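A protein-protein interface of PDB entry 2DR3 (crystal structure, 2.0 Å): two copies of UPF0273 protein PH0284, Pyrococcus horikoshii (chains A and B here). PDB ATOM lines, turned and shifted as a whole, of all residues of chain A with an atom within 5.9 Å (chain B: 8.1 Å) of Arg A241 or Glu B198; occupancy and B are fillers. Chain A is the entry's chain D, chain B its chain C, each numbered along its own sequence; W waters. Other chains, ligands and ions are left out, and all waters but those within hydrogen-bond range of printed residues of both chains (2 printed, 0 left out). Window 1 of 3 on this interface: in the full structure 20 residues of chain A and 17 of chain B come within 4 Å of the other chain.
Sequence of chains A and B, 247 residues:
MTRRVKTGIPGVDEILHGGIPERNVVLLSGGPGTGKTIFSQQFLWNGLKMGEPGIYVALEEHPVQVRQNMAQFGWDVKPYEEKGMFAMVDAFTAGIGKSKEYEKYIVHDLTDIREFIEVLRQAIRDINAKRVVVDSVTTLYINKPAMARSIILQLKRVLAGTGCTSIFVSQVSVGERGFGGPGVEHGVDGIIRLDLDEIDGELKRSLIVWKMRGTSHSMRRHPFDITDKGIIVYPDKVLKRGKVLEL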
ATOM      1  N   ASP A 195      12.744  14.264   3.022  1.00  0.00           N
ATOM      2  CA  ASP A 195      12.323  13.067   3.715  1.00  0.00           C
ATOM      3  C   ASP A 195      11.892  13.284   5.158  1.00  0.00           C
ATOM      4  O   ASP A 195      12.255  14.268   5.801  1.00  0.00           O
ATOM      5  CB  ASP A 195      13.440  12.024   3.658  1.00  0.00           C
ATOM      6  CG  ASP A 195      13.564  11.382   2.281  1.00  0.00           C
ATOM      7  OD1 ASP A 195      12.598  10.703   1.851  1.00  0.00           O
ATOM      8  OD2 ASP A 195      14.618  11.557   1.629  1.00  0.00           O
ATOM      9  N   ASP A 197      11.605  10.534   8.195  1.00  0.00           N
ATOM     10  CA  ASP A 197      11.774   9.142   8.594  1.00  0.00           C
ATOM     11  C   ASP A 197      11.797   8.886  10.091  1.00  0.00           C
ATOM     12  O   ASP A 197      12.354   9.666  10.871  1.00  0.00           O
ATOM     13  CB  ASP A 197      13.061   8.588   7.980  1.00  0.00           C
ATOM     14  CG  ASP A 197      13.117   8.785   6.477  1.00  0.00           C
ATOM     15  OD1 ASP A 197      13.894   9.640   6.001  1.00  0.00           O
ATOM     16  OD2 ASP A 197      12.369   8.086   5.770  1.00  0.00           O
ATOM     17  N   ILE A 199      13.276   7.404  13.050  1.00  0.00           N
ATOM     18  CA  ILE A 199      14.549   6.847  13.468  1.00  0.00           C
ATOM     19  C   ILE A 199      14.589   6.947  14.982  1.00  0.00           C
ATOM     20  O   ILE A 199      14.570   8.046  15.540  1.00  0.00           O
ATOM     21  CB  ILE A 199      15.715   7.616  12.843  1.00  0.00           C
ATOM     22  CG1 ILE A 199      15.652   7.470  11.317  1.00  0.00           C
ATOM     23  CG2 ILE A 199      17.046   7.085  13.384  1.00  0.00           C
ATOM     24  CD1 ILE A 199      16.625   8.355  10.567  1.00  0.00           C
ATOM     25  N   SER A 206      14.967  15.414   6.654  1.00  0.00           N
ATOM     26  CA  SER A 206      16.244  15.486   5.958  1.00  0.00           C
ATOM     27  C   SER A 206      16.059  15.742   4.481  1.00  0.00           C
ATOM     28  O   SER A 206      15.034  15.380   3.884  1.00  0.00           O
ATOM     29  CB  SER A 206      17.076  14.214   6.185  1.00  0.00           C
ATOM     30  OG  SER A 206      16.500  13.070   5.585  1.00  0.00           O
ATOM     31  N   ILE A 208      18.125  15.804   0.538  1.00  0.00           N
ATOM     32  CA  ILE A 208      19.232  15.230  -0.208  1.00  0.00           C
ATOM     33  C   ILE A 208      19.021  15.540  -1.679  1.00  0.00           C
ATOM     34  O   ILE A 208      17.905  15.445  -2.200  1.00  0.00           O
ATOM     35  CB  ILE A 208      19.349  13.695   0.011  1.00  0.00           C
ATOM     36  CG1 ILE A 208      20.652  13.190  -0.615  1.00  0.00           C
ATOM     37  CG2 ILE A 208      18.157  12.965  -0.612  1.00  0.00           C
ATOM     38  CD1 ILE A 208      21.044  11.785  -0.177  1.00  0.00           C
ATOM     39  N   TRP A 210      19.511  14.387  -5.159  1.00  0.00           N
ATOM     40  CA  TRP A 210      19.785  13.176  -5.926  1.00  0.00           C
ATOM     41  C   TRP A 210      20.314  13.503  -7.308  1.00  0.00           C
ATOM     42  O   TRP A 210      21.093  12.746  -7.884  1.00  0.00           O
ATOM     43  CB  TRP A 210      18.512  12.326  -6.083  1.00  0.00           C
ATOM     44  CG  TRP A 210      18.201  11.499  -4.882  1.00  0.00           C
ATOM     45  CD1 TRP A 210      17.441  11.865  -3.804  1.00  0.00           C
ATOM     46  CD2 TRP A 210      18.705  10.191  -4.594  1.00  0.00           C
ATOM     47  NE1 TRP A 210      17.446  10.867  -2.862  1.00  0.00           N
ATOM     48  CE2 TRP A 210      18.216   9.828  -3.321  1.00  0.00           C
ATOM     49  CE3 TRP A 210      19.520   9.289  -5.289  1.00  0.00           C
ATOM     50  CZ2 TRP A 210      18.523   8.595  -2.720  1.00  0.00           C
ATOM     51  CZ3 TRP A 210      19.826   8.062  -4.696  1.00  0.00           C
ATOM     52  CH2 TRP A 210      19.327   7.731  -3.422  1.00  0.00           C
ATOM     53  N   ARG A 221      23.167  13.524   3.022  1.00  0.00           N
ATOM     54  CA  ARG A 221      21.815  13.767   3.532  1.00  0.00           C
ATOM     55  C   ARG A 221      21.921  14.760   4.680  1.00  0.00           C
ATOM     56  O   ARG A 221      22.564  14.486   5.693  1.00  0.00           O
ATOM     57  CB  ARG A 221      21.194  12.454   4.025  1.00  0.00           C
ATOM     58  CG  ARG A 221      19.817  12.599   4.689  1.00  0.00           C
ATOM     59  CD  ARG A 221      19.202  11.236   4.947  1.00  0.00           C
ATOM     60  NE  ARG A 221      18.948  10.516   3.700  1.00  0.00           N
ATOM     61  CZ  ARG A 221      17.985  10.820   2.831  1.00  0.00           C
ATOM     62  NH1 ARG A 221      17.162  11.837   3.068  1.00  0.00           N
ATOM     63  NH2 ARG A 221      17.845  10.106   1.717  1.00  0.00           N
ATOM     64  N   LEU A 239      22.715  13.336   8.309  1.00  0.00           N
ATOM     65  CA  LEU A 239      21.792  12.395   8.938  1.00  0.00           C
ATOM     66  C   LEU A 239      22.032  10.979   8.418  1.00  0.00           C
ATOM     67  O   LEU A 239      22.116  10.749   7.211  1.00  0.00           O
ATOM     68  CB  LEU A 239      20.336  12.797   8.683  1.00  0.00           C
ATOM     69  CG  LEU A 239      19.316  11.824   9.286  1.00  0.00           C
ATOM     70  CD1 LEU A 239      19.562  11.687  10.787  1.00  0.00           C
ATOM     71  CD2 LEU A 239      17.902  12.314   9.015  1.00  0.00           C
ATOM     72  N   LYS A 240      22.126  10.036   9.346  1.00  0.00           N
ATOM     73  CA  LYS A 240      22.378   8.636   9.020  1.00  0.00           C
ATOM     74  C   LYS A 240      21.120   7.801   9.298  1.00  0.00           C
ATOM     75  O   LYS A 240      20.854   7.435  10.444  1.00  0.00           O
ATOM     76  CB  LYS A 240      23.552   8.146   9.873  1.00  0.00           C
ATOM     77  CG  LYS A 240      24.863   7.994   9.139  1.00  0.00           C
ATOM     78  CD  LYS A 240      25.914   8.941   9.720  1.00  0.00           C
ATOM     79  CE  LYS A 240      27.308   8.314   9.676  1.00  0.00           C
ATOM     80  NZ  LYS A 240      28.394   9.319   9.482  1.00  0.00           N
ATOM     81  N   ARG A 241      20.359   7.498   8.245  1.00  0.00           N
ATOM     82  CA  ARG A 241      19.112   6.738   8.374  1.00  0.00           C
ATOM     83  C   ARG A 241      19.266   5.239   8.606  1.00  0.00           C
ATOM     84  O   ARG A 241      18.366   4.599   9.151  1.00  0.00           O
ATOM     85  CB  ARG A 241      18.233   6.935   7.135  1.00  0.00           C
ATOM     86  CG  ARG A 241      17.899   8.374   6.815  1.00  0.00           C
ATOM     87  CD  ARG A 241      16.747   8.443   5.839  1.00  0.00           C
ATOM     88  NE  ARG A 241      16.957   7.600   4.665  1.00  0.00           N
ATOM     89  CZ  ARG A 241      16.059   7.438   3.695  1.00  0.00           C
ATOM     90  NH1 ARG A 241      14.890   8.062   3.760  1.00  0.00           N
ATOM     91  NH2 ARG A 241      16.328   6.657   2.659  1.00  0.00           N
ATOM     92  N   GLY A 242      20.391   4.678   8.182  1.00  0.00           N
ATOM     93  CA  GLY A 242      20.609   3.251   8.347  1.00  0.00           C
ATOM     94  C   GLY A 242      20.520   2.550   7.004  1.00  0.00           C
ATOM     95  O   GLY A 242      20.743   1.340   6.896  1.00  0.00           O
ATOM     96  N   LYS A 243      20.183   3.324   5.975  1.00  0.00           N
ATOM     97  CA  LYS A 243      20.069   2.811   4.614  1.00  0.00           C
ATOM     98  C   LYS A 243      21.140   3.449   3.732  1.00  0.00           C
ATOM     99  O   LYS A 243      21.983   4.200   4.273  1.00  0.00           O
ATOM    100  CB  LYS A 243      18.679   3.113   4.041  1.00  0.00           C
ATOM    101  CG  LYS A 243      17.553   2.298   4.663  1.00  0.00           C
ATOM    102  CD  LYS A 243      16.189   2.738   4.146  1.00  0.00           C
ATOM    103  CE  LYS A 243      15.872   4.157   4.578  1.00  0.00           C
ATOM    104  NZ  LYS A 243      15.904   4.302   6.060  1.00  0.00           N
ATOM    105  N   ASP B 195      25.435   3.074 -10.996  1.00  0.00           N
ATOM    106  CA  ASP B 195      24.604   3.148  -9.801  1.00  0.00           C
ATOM    107  C   ASP B 195      24.920   4.364  -8.924  1.00  0.00           C
ATOM    108  O   ASP B 195      26.012   4.941  -8.997  1.00  0.00           O
ATOM    109  CB  ASP B 195      24.755   1.858  -8.980  1.00  0.00           C
ATOM    110  CG  ASP B 195      24.095   0.659  -9.651  1.00  0.00           C
ATOM    111  OD1 ASP B 195      22.852   0.672  -9.800  1.00  0.00           O
ATOM    112  OD2 ASP B 195      24.816  -0.295 -10.035  1.00  0.00           O
ATOM    113  N   LEU B 196      23.941   4.750  -8.110  1.00  0.00           N
ATOM    114  CA  LEU B 196      24.052   5.880  -7.197  1.00  0.00           C
ATOM    115  C   LEU B 196      23.349   5.397  -5.940  1.00  0.00           C
ATOM    116  O   LEU B 196      22.113   5.370  -5.871  1.00  0.00           O
ATOM    117  CB  LEU B 196      23.340   7.107  -7.775  1.00  0.00           C
ATOM    118  CG  LEU B 196      23.367   8.398  -6.951  1.00  0.00           C
ATOM    119  CD1 LEU B 196      24.777   8.975  -6.884  1.00  0.00           C
ATOM    120  CD2 LEU B 196      22.413   9.406  -7.586  1.00  0.00           C
ATOM    121  N   ASP B 197      24.146   5.003  -4.954  1.00  0.00           N
ATOM    122  CA  ASP B 197      23.617   4.455  -3.719  1.00  0.00           C
ATOM    123  C   ASP B 197      23.946   5.260  -2.477  1.00  0.00           C
ATOM    124  O   ASP B 197      25.044   5.800  -2.346  1.00  0.00           O
ATOM    125  CB  ASP B 197      24.134   3.020  -3.544  1.00  0.00           C
ATOM    126  CG  ASP B 197      23.675   2.095  -4.667  1.00  0.00           C
ATOM    127  OD1 ASP B 197      22.471   1.771  -4.712  1.00  0.00           O
ATOM    128  OD2 ASP B 197      24.504   1.703  -5.512  1.00  0.00           O
ATOM    129  N   GLU B 198      22.980   5.323  -1.568  1.00  0.00           N
ATOM    130  CA  GLU B 198      23.148   6.034  -0.312  1.00  0.00           C
ATOM    131  C   GLU B 198      23.731   5.068   0.711  1.00  0.00           C
ATOM    132  O   GLU B 198      23.178   3.992   0.959  1.00  0.00           O
ATOM    133  CB  GLU B 198      21.805   6.573   0.187  1.00  0.00           C
ATOM    134  CG  GLU B 198      21.876   7.172   1.577  1.00  0.00           C
ATOM    135  CD  GLU B 198      20.583   7.825   2.001  1.00  0.00           C
ATOM    136  OE1 GLU B 198      19.545   7.588   1.343  1.00  0.00           O
ATOM    137  OE2 GLU B 198      20.606   8.571   3.002  1.00  0.00           O
ATOM    138  N   ILE B 199      24.858   5.453   1.294  1.00  0.00           N
ATOM    139  CA  ILE B 199      25.523   4.619   2.292  1.00  0.00           C
ATOM    140  C   ILE B 199      26.058   5.528   3.384  1.00  0.00           C
ATOM    141  O   ILE B 199      26.883   6.400   3.115  1.00  0.00           O
ATOM    142  CB  ILE B 199      26.718   3.848   1.680  1.00  0.00           C
ATOM    143  CG1 ILE B 199      26.331   3.258   0.321  1.00  0.00           C
ATOM    144  CG2 ILE B 199      27.148   2.729   2.630  1.00  0.00           C
ATOM    145  CD1 ILE B 199      27.456   2.522  -0.380  1.00  0.00           C
ATOM    146  N   ASP B 200      25.581   5.340   4.610  1.00  0.00           N
ATOM    147  CA  ASP B 200      26.036   6.162   5.730  1.00  0.00           C
ATOM    148  C   ASP B 200      25.805   7.650   5.505  1.00  0.00           C
ATOM    149  O   ASP B 200      26.687   8.471   5.772  1.00  0.00           O
ATOM    150  CB  ASP B 200      27.524   5.917   5.996  1.00  0.00           C
ATOM    151  CG  ASP B 200      27.767   4.660   6.799  1.00  0.00           C
ATOM    152  OD1 ASP B 200      27.169   4.537   7.891  1.00  0.00           O
ATOM    153  OD2 ASP B 200      28.555   3.799   6.348  1.00  0.00           O
ATOM    154  N   GLY B 201      24.625   7.992   4.999  1.00  0.00           N
ATOM    155  CA  GLY B 201      24.294   9.386   4.773  1.00  0.00           C
ATOM    156  C   GLY B 201      24.970  10.047   3.591  1.00  0.00           C
ATOM    157  O   GLY B 201      24.874  11.255   3.435  1.00  0.00           O
ATOM    158  N   GLU B 202      25.651   9.265   2.760  1.00  0.00           N
ATOM    159  CA  GLU B 202      26.327   9.806   1.580  1.00  0.00           C
ATOM    160  C   GLU B 202      26.022   9.000   0.319  1.00  0.00           C
ATOM    161  O   GLU B 202      25.930   7.776   0.354  1.00  0.00           O
ATOM    162  CB  GLU B 202      27.851   9.852   1.801  1.00  0.00           C
ATOM    163  CG  GLU B 202      28.645  10.352   0.588  1.00  0.00           C
ATOM    164  CD  GLU B 202      30.098  10.693   0.910  1.00  0.00           C
ATOM    165  OE1 GLU B 202      30.810   9.840   1.489  1.00  0.00           O
ATOM    166  OE2 GLU B 202      30.528  11.817   0.574  1.00  0.00           O
ATOM    167  N   LEU B 203      25.860   9.707  -0.793  1.00  0.00           N
ATOM    168  CA  LEU B 203      25.584   9.080  -2.078  1.00  0.00           C
ATOM    169  C   LEU B 203      26.909   8.699  -2.734  1.00  0.00           C
ATOM    170  O   LEU B 203      27.805   9.533  -2.859  1.00  0.00           O
ATOM    171  CB  LEU B 203      24.838  10.050  -2.997  1.00  0.00           C
ATOM    172  CG  LEU B 203      23.438  10.492  -2.564  1.00  0.00           C
ATOM    173  CD1 LEU B 203      22.849  11.391  -3.618  1.00  0.00           C
ATOM    174  CD2 LEU B 203      22.556   9.280  -2.349  1.00  0.00           C
ATOM    175  N   LYS B 204      27.033   7.442  -3.144  1.00  0.00           N
ATOM    176  CA  LYS B 204      28.248   6.980  -3.794  1.00  0.00           C
ATOM    177  C   LYS B 204      27.937   6.451  -5.192  1.00  0.00           C
ATOM    178  O   LYS B 204      26.966   5.716  -5.397  1.00  0.00           O
ATOM    179  CB  LYS B 204      28.918   5.877  -2.966  1.00  0.00           C
ATOM    180  CG  LYS B 204      29.948   6.367  -1.953  1.00  0.00           C
ATOM    181  CD  LYS B 204      29.339   6.681  -0.609  1.00  0.00           C
ATOM    182  CE  LYS B 204      30.425   7.121   0.376  1.00  0.00           C
ATOM    183  NZ  LYS B 204      29.884   7.352   1.751  1.00  0.00           N
ATOM    184  N   ARG B 205      28.761   6.836  -6.156  1.00  0.00           N
ATOM    185  CA  ARG B 205      28.580   6.388  -7.525  1.00  0.00           C
ATOM    186  C   ARG B 205      29.459   5.160  -7.763  1.00  0.00           C
ATOM    187  O   ARG B 205      30.556   5.065  -7.210  1.00  0.00           O
ATOM    188  CB  ARG B 205      28.994   7.497  -8.494  1.00  0.00           C
ATOM    189  CG  ARG B 205      28.375   8.850  -8.204  1.00  0.00           C
ATOM    190  CD  ARG B 205      28.647   9.808  -9.349  1.00  0.00           C
ATOM    191  NE  ARG B 205      28.012  11.106  -9.144  1.00  0.00           N
ATOM    192  CZ  ARG B 205      26.736  11.358  -9.403  1.00  0.00           C
ATOM    193  NH1 ARG B 205      25.954  10.397  -9.879  1.00  0.00           N
ATOM    194  NH2 ARG B 205      26.245  12.576  -9.202  1.00  0.00           N
ATOM    195  N   ARG B 241      31.112  -3.255   0.952  1.00  0.00           N
ATOM    196  CA  ARG B 241      29.900  -3.216   1.767  1.00  0.00           C
ATOM    197  C   ARG B 241      29.160  -1.919   1.513  1.00  0.00           C
ATOM    198  O   ARG B 241      27.987  -1.873   1.170  1.00  0.00           O
ATOM    199  CB  ARG B 241      30.324  -3.239   3.239  1.00  0.00           C
ATOM    200  CG  ARG B 241      31.362  -4.319   3.528  1.00  0.00           C
ATOM    201  CD  ARG B 241      30.847  -5.713   3.156  1.00  0.00           C
ATOM    202  NE  ARG B 241      31.446  -6.737   4.015  1.00  0.00           N
ATOM    203  CZ  ARG B 241      32.788  -6.806   4.054  1.00  0.00           C
ATOM    204  NH1 ARG B 241      33.519  -5.946   3.366  1.00  0.00           N
ATOM    205  NH2 ARG B 241      33.376  -7.759   4.782  1.00  0.00           N
ATOM    206  N   GLY B 242      29.911  -0.850   1.781  1.00  0.00           N
ATOM    207  CA  GLY B 242      29.474   0.506   1.518  1.00  0.00           C
ATOM    208  C   GLY B 242      30.704   1.395   1.621  1.00  0.00           C
ATOM    209  O   GLY B 242      30.650   2.589   1.865  1.00  0.00           O
HETATM  210  O   HOH W   1      23.408  12.842  -9.406  1.00  0.00           O
HETATM  211  O   HOH W   2      22.013   6.967   4.945  1.00  0.00           O
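OE2 of Glu B198 lies within salt-bridge range of NE of Arg A221 (2.6 Å). The side-chain carboxylate (OE1) of Glu B198 lies within salt-bridge range of the guanidinium group (NH2) of Arg A241, 3.6 Å away. The backbone NH (N) of Arg A221 is in hydrogen-bond range of the backbone carbonyl oxygen (O) of Gly B201.
The guanidinium group (NH1) of Arg A221 lies within salt-bridge range of the side-chain carboxylate (OD2) of Asp A195, 2.9 Å away. NH1 of Arg A241 is in salt-bridge range of OD1 of Asp A195, 3.98 Å away. OD1 of Asp A197 lies within salt-bridge range of NH1 of Arg A241. The side-chain hydroxyl of Ser A206 is in hydrogen-bond range of the guanidinium group of Arg A221. O of Arg A221 sits at hydrogen-bond distance from N of Leu A239, at 2.9 Å.
Among the printed residues, merely in contact across the chains: Lys A243 with Glu B198 (3.5 Å), Leu A239 with Gly B201 (3.5 Å), Trp A210 with Leu B196 (3.6 Å), Ile A208 with Leu B203 (3.6 Å), Trp A210 with Leu B203 (3.7 Å), Lys A240 with Asp B200 (3.8 Å) and Lys A243 with Asp B200 (3.8 Å).
Of the printed residues of chain B, Arg A241 touches Glu B198 (3.6 Å). Of the printed residues of chain A, Glu B198 touches Arg A221, Arg A241 and Lys A243. Printed residues of chain B within 4 Å of Trp A210: Leu B196 (3.6 Å) and Leu B203 (3.7 Å). Printed residues of chain B within 4 Å of Lys A243: Glu B198 and Asp B200. Of the printed residues of chain A, Asp B200 touches Lys A240 (3.8 Å) and Lys A243 (3.8 Å). Printed residues of chain A within 4 Å of Leu B203: Ile A208 and Trp A210. Asp A197 touches none of the printed residues of chain B. Asp B197 touches none of the printed residues of chain A. The nearest printed residue of chain B that does not touch Lys A240 is Gly B201 (4.1 Å).
Hydrophobic or aromatic side chains of chain B within 4 Å of the printed part of chain A: Leu B196 and Leu B203. Among the printed residues, 10 pairs touch across the chains.
Positions printed for both chains: 195, 197, 199, 241 and 242. Of the 10 pairs that touch across the chains among the printed residues, none has its exchanged pair printed and touching as well.
Water W1 bridges the backbone carbonyl oxygen of Trp A210 (2.8 Å) and the guanidinium group of Arg B205 (2.9 Å). Water W2 lies within hydrogen-bond range of the backbone NH of Gly B201 (2.8 Å), the backbone carbonyl oxygen of Lys A243 (2.8 Å) and the side-chain carboxylate of Glu B198 (2.9 Å).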
